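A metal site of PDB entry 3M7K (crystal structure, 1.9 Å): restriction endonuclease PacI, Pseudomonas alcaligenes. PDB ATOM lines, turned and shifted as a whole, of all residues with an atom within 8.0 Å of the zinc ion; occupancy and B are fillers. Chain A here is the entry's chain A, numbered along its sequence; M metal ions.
The backbone NH of Ile 111 lies close to the side-chain sulfur of Cys 109. The backbone carbonyl oxygen (O) of Cys 66 sits close to the side-chain hydroxyl (OG) of Ser 133 (3.2 Å). The backbone NH (N) of Cys 63 lies within hydrogen-bond range of the backbone carbonyl oxygen (O) of Ile 68, at 2.8 Å. The side-chain sulfur (SG) of Cys 66 sits close to the backbone NH (N) of Ile 68. The side-chain sulfur of Cys 66 lies close to the indole nitrogen of Trp 136 (3.2 Å). The side-chain sulfur of Cys 63 lies close to the backbone NH of Tyr 65, 3.4 Å away.
Four residues have an atom within 4 Å of the zinc ion: Cys 63, Cys 66, Cys 109 and Cys 112. The nearest printed residue that does not touch the zinc ion is Ile 68 (4.3 Å).
The zinc ion is bound by the side-chain sulfur (SG) of Cys 66, the side-chain sulfur (SG) of Cys 109, the side-chain sulfur (SG) of Cys 112 and the side-chain sulfur (SG) of Cys 63.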
ATOM      1  N   HIS A  62      20.509  -2.029 -14.771  1.00  0.00           N
ATOM      2  CA  HIS A  62      21.677  -2.057 -15.663  1.00  0.00           C
ATOM      3  C   HIS A  62      21.393  -1.047 -16.754  1.00  0.00           C
ATOM      4  O   HIS A  62      20.242  -0.873 -17.160  1.00  0.00           O
ATOM      5  CB  HIS A  62      21.850  -3.436 -16.329  1.00  0.00           C
ATOM      6  CG  HIS A  62      22.211  -4.536 -15.385  1.00  0.00           C
ATOM      7  ND1 HIS A  62      21.266  -5.204 -14.626  1.00  0.00           N
ATOM      8  CD2 HIS A  62      23.401  -5.105 -15.100  1.00  0.00           C
ATOM      9  CE1 HIS A  62      21.872  -6.121 -13.897  1.00  0.00           C
ATOM     10  NE2 HIS A  62      23.165  -6.089 -14.160  1.00  0.00           N
ATOM     11  N   CYS A  63      22.448  -0.399 -17.245  1.00  0.00           N
ATOM     12  CA  CYS A  63      22.308   0.557 -18.313  1.00  0.00           C
ATOM     13  C   CYS A  63      21.831  -0.181 -19.562  1.00  0.00           C
ATOM     14  O   CYS A  63      22.378  -1.221 -19.916  1.00  0.00           O
ATOM     15  CB  CYS A  63      23.649   1.234 -18.583  1.00  0.00           C
ATOM     16  SG  CYS A  63      23.694   2.261 -20.103  1.00  0.00           S
ATOM     17  N   GLY A  64      20.815   0.353 -20.223  1.00  0.00           N
ATOM     18  CA  GLY A  64      20.213  -0.265 -21.398  1.00  0.00           C
ATOM     19  C   GLY A  64      21.048  -0.160 -22.670  1.00  0.00           C
ATOM     20  O   GLY A  64      20.678  -0.740 -23.698  1.00  0.00           O
ATOM     21  N   TYR A  65      22.158   0.587 -22.624  1.00  0.00           N
ATOM     22  CA  TYR A  65      23.081   0.668 -23.740  1.00  0.00           C
ATOM     23  C   TYR A  65      24.341  -0.154 -23.540  1.00  0.00           C
ATOM     24  O   TYR A  65      24.668  -0.972 -24.387  1.00  0.00           O
ATOM     25  CB  TYR A  65      23.457   2.116 -24.074  1.00  0.00           C
ATOM     26  CG  TYR A  65      22.253   2.892 -24.533  1.00  0.00           C
ATOM     27  CD1 TYR A  65      21.730   3.934 -23.767  1.00  0.00           C
ATOM     28  CD2 TYR A  65      21.584   2.529 -25.717  1.00  0.00           C
ATOM     29  CE1 TYR A  65      20.600   4.644 -24.194  1.00  0.00           C
ATOM     30  CE2 TYR A  65      20.457   3.206 -26.144  1.00  0.00           C
ATOM     31  CZ  TYR A  65      19.983   4.255 -25.383  1.00  0.00           C
ATOM     32  OH  TYR A  65      18.863   4.920 -25.807  1.00  0.00           O
ATOM     33  N   CYS A  66      25.051   0.068 -22.425  1.00  0.00           N
ATOM     34  CA  CYS A  66      26.325  -0.639 -22.208  1.00  0.00           C
ATOM     35  C   CYS A  66      26.226  -1.846 -21.288  1.00  0.00           C
ATOM     36  O   CYS A  66      27.182  -2.616 -21.184  1.00  0.00           O
ATOM     37  CB  CYS A  66      27.392   0.322 -21.671  1.00  0.00           C
ATOM     38  SG  CYS A  66      27.110   0.875 -19.954  1.00  0.00           S
ATOM     39  N   GLY A  67      25.106  -1.987 -20.589  1.00  0.00           N
ATOM     40  CA  GLY A  67      24.887  -3.160 -19.740  1.00  0.00           C
ATOM     41  C   GLY A  67      25.530  -3.046 -18.371  1.00  0.00           C
ATOM     42  O   GLY A  67      25.407  -3.951 -17.548  1.00  0.00           O
ATOM     43  N   ILE A  68      26.193  -1.937 -18.073  1.00  0.00           N
ATOM     44  CA  ILE A  68      26.848  -1.855 -16.774  1.00  0.00           C
ATOM     45  C   ILE A  68      25.786  -1.874 -15.652  1.00  0.00           C
ATOM     46  O   ILE A  68      24.704  -1.302 -15.808  1.00  0.00           O
ATOM     47  CB  ILE A  68      27.766  -0.620 -16.664  1.00  0.00           C
ATOM     48  CG1 ILE A  68      28.742  -0.810 -15.480  1.00  0.00           C
ATOM     49  CG2 ILE A  68      26.939   0.684 -16.514  1.00  0.00           C
ATOM     50  CD1 ILE A  68      29.884   0.136 -15.494  1.00  0.00           C
ATOM     51  N   SER A  69      26.097  -2.553 -14.549  1.00  0.00           N
ATOM     52  CA  SER A  69      25.193  -2.616 -13.399  1.00  0.00           C
ATOM     53  C   SER A  69      25.333  -1.308 -12.623  1.00  0.00           C
ATOM     54  O   SER A  69      26.339  -0.596 -12.752  1.00  0.00           O
ATOM     55  CB  SER A  69      25.546  -3.788 -12.490  1.00  0.00           C
ATOM     56  OG  SER A  69      26.809  -3.558 -11.861  1.00  0.00           O
ATOM     57  N   PHE A  73      28.730   0.844 -12.244  1.00  0.00           N
ATOM     58  CA  PHE A  73      28.843   2.258 -12.511  1.00  0.00           C
ATOM     59  C   PHE A  73      29.296   3.068 -11.298  1.00  0.00           C
ATOM     60  O   PHE A  73      30.105   3.975 -11.429  1.00  0.00           O
ATOM     61  CB  PHE A  73      27.545   2.829 -13.070  1.00  0.00           C
ATOM     62  CG  PHE A  73      27.702   4.204 -13.639  1.00  0.00           C
ATOM     63  CD1 PHE A  73      28.338   4.392 -14.864  1.00  0.00           C
ATOM     64  CD2 PHE A  73      27.227   5.317 -12.941  1.00  0.00           C
ATOM     65  CE1 PHE A  73      28.508   5.668 -15.410  1.00  0.00           C
ATOM     66  CE2 PHE A  73      27.374   6.634 -13.507  1.00  0.00           C
ATOM     67  CZ  PHE A  73      28.034   6.778 -14.729  1.00  0.00           C
ATOM     68  N   LEU A  76      32.940   3.232 -10.852  1.00  0.00           N
ATOM     69  CA  LEU A  76      33.697   4.124 -11.715  1.00  0.00           C
ATOM     70  C   LEU A  76      34.003   5.460 -11.057  1.00  0.00           C
ATOM     71  O   LEU A  76      34.845   6.202 -11.528  1.00  0.00           O
ATOM     72  CB  LEU A  76      32.937   4.353 -13.052  1.00  0.00           C
ATOM     73  CG  LEU A  76      32.898   3.147 -13.997  1.00  0.00           C
ATOM     74  CD1 LEU A  76      32.028   3.442 -15.192  1.00  0.00           C
ATOM     75  CD2 LEU A  76      34.316   2.807 -14.434  1.00  0.00           C
ATOM     76  N   LEU A  89      21.732   4.850 -11.624  1.00  0.00           N
ATOM     77  CA  LEU A  89      21.544   4.977 -13.059  1.00  0.00           C
ATOM     78  C   LEU A  89      20.400   5.912 -13.353  1.00  0.00           C
ATOM     79  O   LEU A  89      19.447   5.984 -12.578  1.00  0.00           O
ATOM     80  CB  LEU A  89      21.289   3.611 -13.692  1.00  0.00           C
ATOM     81  CG  LEU A  89      22.398   2.593 -13.440  1.00  0.00           C
ATOM     82  CD1 LEU A  89      22.084   1.336 -14.193  1.00  0.00           C
ATOM     83  CD2 LEU A  89      23.785   3.109 -13.851  1.00  0.00           C
ATOM     84  N   LEU A 107      16.589   3.022 -19.239  1.00  0.00           N
ATOM     85  CA  LEU A 107      17.564   3.238 -18.179  1.00  0.00           C
ATOM     86  C   LEU A 107      18.920   3.426 -18.838  1.00  0.00           C
ATOM     87  O   LEU A 107      19.260   2.685 -19.772  1.00  0.00           O
ATOM     88  CB  LEU A 107      17.612   2.047 -17.242  1.00  0.00           C
ATOM     89  CG  LEU A 107      17.988   2.157 -15.775  1.00  0.00           C
ATOM     90  CD1 LEU A 107      17.126   3.150 -14.974  1.00  0.00           C
ATOM     91  CD2 LEU A 107      17.911   0.735 -15.189  1.00  0.00           C
ATOM     92  N   ALA A 108      19.677   4.406 -18.374  1.00  0.00           N
ATOM     93  CA  ALA A 108      21.002   4.665 -18.911  1.00  0.00           C
ATOM     94  C   ALA A 108      21.970   5.204 -17.850  1.00  0.00           C
ATOM     95  O   ALA A 108      21.592   6.052 -17.029  1.00  0.00           O
ATOM     96  CB  ALA A 108      20.930   5.643 -20.102  1.00  0.00           C
ATOM     97  N   CYS A 109      23.215   4.749 -17.880  1.00  0.00           N
ATOM     98  CA  CYS A 109      24.232   5.303 -17.000  1.00  0.00           C
ATOM     99  C   CYS A 109      24.578   6.685 -17.525  1.00  0.00           C
ATOM    100  O   CYS A 109      24.323   7.007 -18.708  1.00  0.00           O
ATOM    101  CB  CYS A 109      25.497   4.405 -16.940  1.00  0.00           C
ATOM    102  SG  CYS A 109      26.608   4.438 -18.425  1.00  0.00           S
ATOM    103  N   PHE A 110      25.115   7.533 -16.671  1.00  0.00           N
ATOM    104  CA  PHE A 110      25.376   8.929 -17.055  1.00  0.00           C
ATOM    105  C   PHE A 110      26.430   9.049 -18.159  1.00  0.00           C
ATOM    106  O   PHE A 110      26.425  10.024 -18.942  1.00  0.00           O
ATOM    107  CB  PHE A 110      25.800   9.739 -15.827  1.00  0.00           C
ATOM    108  CG  PHE A 110      25.661  11.246 -15.988  1.00  0.00           C
ATOM    109  CD1 PHE A 110      24.596  11.799 -16.696  1.00  0.00           C
ATOM    110  CD2 PHE A 110      26.583  12.106 -15.384  1.00  0.00           C
ATOM    111  CE1 PHE A 110      24.460  13.164 -16.839  1.00  0.00           C
ATOM    112  CE2 PHE A 110      26.449  13.507 -15.487  1.00  0.00           C
ATOM    113  CZ  PHE A 110      25.379  14.044 -16.210  1.00  0.00           C
ATOM    114  N   ILE A 111      27.325   8.061 -18.257  1.00  0.00           N
ATOM    115  CA  ILE A 111      28.295   8.058 -19.352  1.00  0.00           C
ATOM    116  C   ILE A 111      27.585   7.876 -20.708  1.00  0.00           C
ATOM    117  O   ILE A 111      27.798   8.667 -21.625  1.00  0.00           O
ATOM    118  CB  ILE A 111      29.448   7.028 -19.137  1.00  0.00           C
ATOM    119  CG1 ILE A 111      30.409   7.543 -18.049  1.00  0.00           C
ATOM    120  CG2 ILE A 111      30.212   6.757 -20.451  1.00  0.00           C
ATOM    121  CD1 ILE A 111      31.556   6.576 -17.621  1.00  0.00           C
ATOM    122  N   CYS A 112      26.738   6.852 -20.824  1.00  0.00           N
ATOM    123  CA  CYS A 112      26.050   6.622 -22.101  1.00  0.00           C
ATOM    124  C   CYS A 112      25.043   7.729 -22.380  1.00  0.00           C
ATOM    125  O   CYS A 112      24.845   8.129 -23.532  1.00  0.00           O
ATOM    126  CB  CYS A 112      25.326   5.266 -22.088  1.00  0.00           C
ATOM    127  SG  CYS A 112      26.467   3.873 -22.137  1.00  0.00           S
ATOM    128  N   ASN A 113      24.376   8.210 -21.339  1.00  0.00           N
ATOM    129  CA  ASN A 113      23.383   9.265 -21.532  1.00  0.00           C
ATOM    130  C   ASN A 113      24.049  10.495 -22.167  1.00  0.00           C
ATOM    131  O   ASN A 113      23.488  11.098 -23.113  1.00  0.00           O
ATOM    132  CB  ASN A 113      22.682   9.643 -20.196  1.00  0.00           C
ATOM    133  CG  ASN A 113      21.176   9.889 -20.381  1.00  0.00           C
ATOM    134  OD1 ASN A 113      20.681   9.970 -21.528  1.00  0.00           O
ATOM    135  ND2 ASN A 113      20.461  10.003 -19.285  1.00  0.00           N
ATOM    136  N   ILE A 115      26.991  10.605 -23.770  1.00  0.00           N
ATOM    137  CA  ILE A 115      27.493  10.238 -25.119  1.00  0.00           C
ATOM    138  C   ILE A 115      26.426  10.336 -26.199  1.00  0.00           C
ATOM    139  O   ILE A 115      26.617  11.010 -27.245  1.00  0.00           O
ATOM    140  CB  ILE A 115      28.183   8.849 -25.100  1.00  0.00           C
ATOM    141  CG1 ILE A 115      29.472   8.988 -24.279  1.00  0.00           C
ATOM    142  CG2 ILE A 115      28.465   8.335 -26.530  1.00  0.00           C
ATOM    143  CD1 ILE A 115      30.189   7.649 -23.968  1.00  0.00           C
ATOM    144  N   MET A 125      22.891   4.246 -30.769  1.00  0.00           N
ATOM    145  CA  MET A 125      23.506   4.153 -29.438  1.00  0.00           C
ATOM    146  C   MET A 125      23.605   2.705 -28.926  1.00  0.00           C
ATOM    147  O   MET A 125      24.516   2.368 -28.138  1.00  0.00           O
ATOM    148  CB  MET A 125      22.770   5.041 -28.420  1.00  0.00           C
ATOM    149  CG  MET A 125      23.568   5.205 -27.103  1.00  0.00           C
ATOM    150  SD  MET A 125      25.170   6.077 -27.314  1.00  0.00           S
ATOM    151  CE  MET A 125      26.055   5.584 -25.823  1.00  0.00           C
ATOM    152  N   GLY A 129      26.910   1.426 -27.372  1.00  0.00           N
ATOM    153  CA  GLY A 129      26.806   0.691 -26.095  1.00  0.00           C
ATOM    154  C   GLY A 129      27.610  -0.614 -26.042  1.00  0.00           C
ATOM    155  O   GLY A 129      28.301  -0.876 -25.038  1.00  0.00           O
ATOM    156  N   ILE A 132      31.175   0.322 -25.659  1.00  0.00           N
ATOM    157  CA  ILE A 132      31.411   0.783 -24.297  1.00  0.00           C
ATOM    158  C   ILE A 132      31.458  -0.403 -23.326  1.00  0.00           C
ATOM    159  O   ILE A 132      32.301  -0.438 -22.438  1.00  0.00           O
ATOM    160  CB  ILE A 132      30.349   1.828 -23.866  1.00  0.00           C
ATOM    161  CG1 ILE A 132      30.476   3.102 -24.713  1.00  0.00           C
ATOM    162  CG2 ILE A 132      30.488   2.186 -22.382  1.00  0.00           C
ATOM    163  CD1 ILE A 132      29.224   3.977 -24.721  1.00  0.00           C
ATOM    164  N   SER A 133      30.506  -1.331 -23.475  1.00  0.00           N
ATOM    165  CA  SER A 133      30.498  -2.614 -22.726  1.00  0.00           C
ATOM    166  C   SER A 133      31.844  -3.360 -22.827  1.00  0.00           C
ATOM    167  O   SER A 133      32.296  -3.943 -21.848  1.00  0.00           O
ATOM    168  CB  SER A 133      29.338  -3.510 -23.184  1.00  0.00           C
ATOM    169  OG  SER A 133      29.245  -4.709 -22.418  1.00  0.00           O
ATOM    170  N   TRP A 136      34.305  -1.732 -20.454  1.00  0.00           N
ATOM    171  CA  TRP A 136      34.053  -2.139 -19.073  1.00  0.00           C
ATOM    172  C   TRP A 136      34.566  -3.561 -18.836  1.00  0.00           C
ATOM    173  O   TRP A 136      35.322  -3.799 -17.890  1.00  0.00           O
ATOM    174  CB  TRP A 136      32.563  -2.051 -18.705  1.00  0.00           C
ATOM    175  CG  TRP A 136      31.861  -0.682 -18.915  1.00  0.00           C
ATOM    176  CD1 TRP A 136      30.542  -0.503 -19.203  1.00  0.00           C
ATOM    177  CD2 TRP A 136      32.434   0.635 -18.831  1.00  0.00           C
ATOM    178  NE1 TRP A 136      30.256   0.830 -19.308  1.00  0.00           N
ATOM    179  CE2 TRP A 136      31.396   1.552 -19.093  1.00  0.00           C
ATOM    180  CE3 TRP A 136      33.724   1.120 -18.582  1.00  0.00           C
ATOM    181  CZ2 TRP A 136      31.599   2.954 -19.113  1.00  0.00           C
ATOM    182  CZ3 TRP A 136      33.934   2.504 -18.586  1.00  0.00           C
ATOM    183  CH2 TRP A 136      32.869   3.410 -18.853  1.00  0.00           C
HETATM  184 ZN    ZN M   1      26.020   2.875 -20.063  1.00  0.00          ZN
